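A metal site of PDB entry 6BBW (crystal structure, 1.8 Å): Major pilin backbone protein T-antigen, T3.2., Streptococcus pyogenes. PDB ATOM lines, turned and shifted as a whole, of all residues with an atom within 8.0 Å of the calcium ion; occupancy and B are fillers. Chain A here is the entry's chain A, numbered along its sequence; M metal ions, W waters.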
ATOM      1  N   THR A 157      -7.351 -10.095   7.071  1.00  0.00           N
ATOM      2  CA  THR A 157      -8.140  -8.896   7.300  1.00  0.00           C
ATOM      3  C   THR A 157      -8.922  -8.632   6.028  1.00  0.00           C
ATOM      4  O   THR A 157      -9.095  -9.530   5.218  1.00  0.00           O
ATOM      5  CB  THR A 157      -7.263  -7.740   7.791  1.00  0.00           C
ATOM      6  OG1 THR A 157      -8.070  -6.603   8.133  1.00  0.00           O
ATOM      7  CG2 THR A 157      -6.212  -7.343   6.753  1.00  0.00           C
ATOM      8  N   SER A 158      -9.467  -7.423   5.883  1.00  0.00           N
ATOM      9  CA  SER A 158     -10.346  -7.109   4.789  1.00  0.00           C
ATOM     10  C   SER A 158     -10.326  -5.634   4.440  1.00  0.00           C
ATOM     11  O   SER A 158      -9.940  -4.784   5.248  1.00  0.00           O
ATOM     12  CB  SER A 158     -11.786  -7.526   5.124  1.00  0.00           C
ATOM     13  OG  SER A 158     -12.223  -6.777   6.230  1.00  0.00           O
ATOM     14  N   TYR A 232      -1.621  -1.106   0.795  1.00  0.00           N
ATOM     15  CA  TYR A 232      -2.419  -0.859  -0.372  1.00  0.00           C
ATOM     16  C   TYR A 232      -2.617   0.648  -0.572  1.00  0.00           C
ATOM     17  O   TYR A 232      -2.436   1.449   0.360  1.00  0.00           O
ATOM     18  CB  TYR A 232      -3.769  -1.578  -0.259  1.00  0.00           C
ATOM     19  CG  TYR A 232      -4.677  -1.050   0.838  1.00  0.00           C
ATOM     20  CD1 TYR A 232      -5.496   0.043   0.615  1.00  0.00           C
ATOM     21  CD2 TYR A 232      -4.736  -1.672   2.099  1.00  0.00           C
ATOM     22  CE1 TYR A 232      -6.312   0.541   1.602  1.00  0.00           C
ATOM     23  CE2 TYR A 232      -5.552  -1.194   3.093  1.00  0.00           C
ATOM     24  CZ  TYR A 232      -6.352  -0.089   2.841  1.00  0.00           C
ATOM     25  OH  TYR A 232      -7.175   0.432   3.788  1.00  0.00           O
ATOM     26  N   LEU A 250     -11.546   6.619   5.928  1.00  0.00           N
ATOM     27  CA  LEU A 250     -11.240   5.255   6.382  1.00  0.00           C
ATOM     28  C   LEU A 250     -11.791   5.005   7.788  1.00  0.00           C
ATOM     29  O   LEU A 250     -11.595   5.829   8.709  1.00  0.00           O
ATOM     30  CB  LEU A 250      -9.725   5.027   6.379  1.00  0.00           C
ATOM     31  CG  LEU A 250      -9.162   3.761   7.039  1.00  0.00           C
ATOM     32  CD1 LEU A 250      -9.630   2.515   6.319  1.00  0.00           C
ATOM     33  CD2 LEU A 250      -7.641   3.842   7.069  1.00  0.00           C
ATOM     34  N   LYS A 251     -12.457   3.871   7.950  1.00  0.00           N
ATOM     35  CA  LYS A 251     -12.964   3.394   9.242  1.00  0.00           C
ATOM     36  C   LYS A 251     -12.372   2.008   9.490  1.00  0.00           C
ATOM     37  O   LYS A 251     -12.463   1.132   8.639  1.00  0.00           O
ATOM     38  CB  LYS A 251     -14.492   3.321   9.221  1.00  0.00           C
ATOM     39  CG  LYS A 251     -15.163   2.964  10.545  1.00  0.00           C
ATOM     40  CD  LYS A 251     -16.641   3.344  10.517  1.00  0.00           C
ATOM     41  CE  LYS A 251     -17.439   2.616  11.579  1.00  0.00           C
ATOM     42  NZ  LYS A 251     -18.006   1.335  11.037  1.00  0.00           N
ATOM     43  N   GLU A 252     -11.792   1.804  10.672  1.00  0.00           N
ATOM     44  CA  GLU A 252     -11.186   0.542  11.044  1.00  0.00           C
ATOM     45  C   GLU A 252     -11.959  -0.085  12.194  1.00  0.00           C
ATOM     46  O   GLU A 252     -12.216   0.565  13.203  1.00  0.00           O
ATOM     47  CB  GLU A 252      -9.737   0.785  11.443  1.00  0.00           C
ATOM     48  CG  GLU A 252      -8.888   1.192  10.258  1.00  0.00           C
ATOM     49  CD  GLU A 252      -7.416   1.193  10.563  1.00  0.00           C
ATOM     50  OE1 GLU A 252      -6.745   0.159  10.385  1.00  0.00           O
ATOM     51  OE2 GLU A 252      -6.915   2.237  11.021  1.00  0.00           O
ATOM     52  N   GLY A 253     -12.368  -1.350  12.012  1.00  0.00           N
ATOM     53  CA  GLY A 253     -13.293  -2.013  12.928  1.00  0.00           C
ATOM     54  C   GLY A 253     -14.520  -1.173  13.239  1.00  0.00           C
ATOM     55  O   GLY A 253     -15.108  -0.549  12.341  1.00  0.00           O
ATOM     56  N   LYS A 258     -11.815   8.462   9.843  1.00  0.00           N
ATOM     57  CA  LYS A 258     -10.834   9.519   9.633  1.00  0.00           C
ATOM     58  C   LYS A 258     -10.603   9.735   8.135  1.00  0.00           C
ATOM     59  O   LYS A 258     -11.008   8.892   7.316  1.00  0.00           O
ATOM     60  CB  LYS A 258      -9.496   9.209  10.335  1.00  0.00           C
ATOM     61  CG  LYS A 258      -8.785   7.927   9.911  1.00  0.00           C
ATOM     62  CD  LYS A 258      -9.008   6.826  10.925  1.00  0.00           C
ATOM     63  CE  LYS A 258      -8.260   5.558  10.576  1.00  0.00           C
ATOM     64  NZ  LYS A 258      -8.376   4.559  11.676  1.00  0.00           N
ATOM     65  N   GLN A 266      -1.649   2.486   2.788  1.00  0.00           N
ATOM     66  CA  GLN A 266      -2.246   2.117   4.095  1.00  0.00           C
ATOM     67  C   GLN A 266      -1.786   0.705   4.394  1.00  0.00           C
ATOM     68  O   GLN A 266      -1.911  -0.152   3.540  1.00  0.00           O
ATOM     69  CB  GLN A 266      -3.767   2.155   3.998  1.00  0.00           C
ATOM     70  CG  GLN A 266      -4.554   1.700   5.236  1.00  0.00           C
ATOM     71  CD  GLN A 266      -4.291   2.537   6.456  1.00  0.00           C
ATOM     72  OE1 GLN A 266      -3.957   3.715   6.358  1.00  0.00           O
ATOM     73  NE2 GLN A 266      -4.480   1.940   7.639  1.00  0.00           N
ATOM     74  N   LYS A 267      -1.254   0.455   5.600  1.00  0.00           N
ATOM     75  CA  LYS A 267      -0.790  -0.879   5.966  1.00  0.00           C
ATOM     76  C   LYS A 267      -1.951  -1.706   6.504  1.00  0.00           C
ATOM     77  O   LYS A 267      -2.732  -1.209   7.291  1.00  0.00           O
ATOM     78  CB  LYS A 267       0.327  -0.822   7.003  1.00  0.00           C
ATOM     79  CG  LYS A 267       0.983  -2.175   7.240  1.00  0.00           C
ATOM     80  CD  LYS A 267       2.205  -2.023   8.129  1.00  0.00           C
ATOM     81  CE  LYS A 267       2.935  -3.340   8.212  1.00  0.00           C
ATOM     82  NZ  LYS A 267       4.167  -3.280   9.048  1.00  0.00           N
ATOM     83  N   THR A 268      -2.059  -2.950   6.043  1.00  0.00           N
ATOM     84  CA  THR A 268      -3.104  -3.861   6.542  1.00  0.00           C
ATOM     85  C   THR A 268      -2.691  -4.419   7.904  1.00  0.00           C
ATOM     86  O   THR A 268      -1.526  -4.745   8.119  1.00  0.00           O
ATOM     87  CB  THR A 268      -3.394  -5.016   5.566  1.00  0.00           C
ATOM     88  OG1 THR A 268      -2.266  -5.891   5.434  1.00  0.00           O
ATOM     89  CG2 THR A 268      -3.771  -4.474   4.215  1.00  0.00           C
ATOM     90  N   ASP A 269      -3.651  -4.492   8.816  1.00  0.00           N
ATOM     91  CA  ASP A 269      -3.432  -5.011  10.159  1.00  0.00           C
ATOM     92  C   ASP A 269      -4.704  -5.760  10.597  1.00  0.00           C
ATOM     93  O   ASP A 269      -5.505  -6.074   9.742  1.00  0.00           O
ATOM     94  CB  ASP A 269      -3.007  -3.884  11.105  1.00  0.00           C
ATOM     95  CG  ASP A 269      -4.078  -2.829  11.322  1.00  0.00           C
ATOM     96  OD1 ASP A 269      -5.184  -2.880  10.713  1.00  0.00           O
ATOM     97  OD2 ASP A 269      -3.801  -1.927  12.136  1.00  0.00           O
ATOM     98  N   GLU A 270      -4.917  -6.008  11.888  1.00  0.00           N
ATOM     99  CA  GLU A 270      -6.033  -6.866  12.334  1.00  0.00           C
ATOM    100  C   GLU A 270      -7.389  -6.180  12.474  1.00  0.00           C
ATOM    101  O   GLU A 270      -8.342  -6.768  13.009  1.00  0.00           O
ATOM    102  CB  GLU A 270      -5.702  -7.580  13.660  1.00  0.00           C
ATOM    103  CG  GLU A 270      -4.778  -8.775  13.496  1.00  0.00           C
ATOM    104  CD  GLU A 270      -3.308  -8.414  13.480  1.00  0.00           C
ATOM    105  OE1 GLU A 270      -2.967  -7.236  13.284  1.00  0.00           O
ATOM    106  OE2 GLU A 270      -2.494  -9.330  13.679  1.00  0.00           O
ATOM    107  N   SER A 271      -7.518  -4.931  12.016  1.00  0.00           N
ATOM    108  CA  SER A 271      -8.820  -4.283  12.034  1.00  0.00           C
ATOM    109  C   SER A 271      -9.330  -4.208  10.610  1.00  0.00           C
ATOM    110  O   SER A 271      -8.610  -3.774   9.725  1.00  0.00           O
ATOM    111  CB  SER A 271      -8.754  -2.872  12.620  1.00  0.00           C
ATOM    112  OG  SER A 271      -7.808  -2.082  11.923  1.00  0.00           O
ATOM    113  N   ALA A 272     -10.564  -4.623  10.396  1.00  0.00           N
ATOM    114  CA  ALA A 272     -11.184  -4.549   9.075  1.00  0.00           C
ATOM    115  C   ALA A 272     -11.235  -3.095   8.593  1.00  0.00           C
ATOM    116  O   ALA A 272     -11.538  -2.196   9.385  1.00  0.00           O
ATOM    117  CB  ALA A 272     -12.564  -5.140   9.133  1.00  0.00           C
ATOM    118  N   ASP A 273     -10.932  -2.866   7.317  1.00  0.00           N
ATOM    119  CA  ASP A 273     -10.928  -1.530   6.753  1.00  0.00           C
ATOM    120  C   ASP A 273     -12.145  -1.314   5.864  1.00  0.00           C
ATOM    121  O   ASP A 273     -12.497  -2.165   5.041  1.00  0.00           O
ATOM    122  CB  ASP A 273      -9.690  -1.273   5.882  1.00  0.00           C
ATOM    123  CG  ASP A 273      -8.398  -1.174   6.661  1.00  0.00           C
ATOM    124  OD1 ASP A 273      -8.376  -1.268   7.904  1.00  0.00           O
ATOM    125  OD2 ASP A 273      -7.360  -0.970   5.991  1.00  0.00           O
ATOM    126  N   GLU A 274     -12.736  -0.136   5.997  1.00  0.00           N
ATOM    127  CA  GLU A 274     -13.782   0.332   5.085  1.00  0.00           C
ATOM    128  C   GLU A 274     -13.464   1.737   4.654  1.00  0.00           C
ATOM    129  O   GLU A 274     -13.289   2.621   5.491  1.00  0.00           O
ATOM    130  CB  GLU A 274     -15.160   0.276   5.737  1.00  0.00           C
ATOM    131  CG  GLU A 274     -15.568  -1.136   6.097  1.00  0.00           C
ATOM    132  CD  GLU A 274     -17.050  -1.295   6.426  1.00  0.00           C
ATOM    133  OE1 GLU A 274     -17.824  -0.325   6.233  1.00  0.00           O
ATOM    134  OE2 GLU A 274     -17.440  -2.412   6.855  1.00  0.00           O
HETATM  135 CA    CA M   1      -6.934  -1.976   9.531  1.00  0.00          CA
HETATM  136  O   HOH W   1      -6.429  -3.959   7.957  1.00  0.00           O
HETATM  137  O   HOH W   2      -5.359  -0.943   7.937  1.00  0.00           O
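OE2 of Glu 252 is in salt-bridge range of NZ of Lys 258, 2.8 Å away. The side-chain carboxylate (OD2) of Asp 273 sits at hydrogen-bond distance from the side-chain hydroxyl (OH) of Tyr 232 (2.6 Å). The side-chain hydroxyl of Thr 157 sits close to the backbone carbonyl oxygen of Ser 271 (3.3 Å). OG1 of Thr 157 lies within hydrogen-bond range of O of Asp 269, at 3.1 Å. The backbone NH of Asp 273 lies within hydrogen-bond range of the backbone carbonyl oxygen of Ser 158, at 3.0 Å.
Water W2 lies within hydrogen-bond range of O of Lys 267 (2.7 Å), OD2 of Asp 273 (2.8 Å) and NE2 of Gln 266 (3.0 Å). Water W1 bridges the backbone carbonyl oxygen of Asp 269 (2.9 Å) and the side-chain hydroxyl of Thr 157 (3.1 Å).
Of the 17 residues printed, 4 come within 4 Å of the calcium ion. The nearest printed residue that does not touch the calcium ion is Ala 272 (4.5 Å).
The calcium ion is bound by OD1 of Asp 273 (2.3 Å), OD1 of Asp 269 (2.3 Å), OE1 of Glu 252 (2.3 Å), O of Ser 271 (2.5 Å), water W2 (2.5 Å), OG of Ser 271 (2.5 Å) and water W1 (2.6 Å). The calcium ion has seven donor atoms within binding distance.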
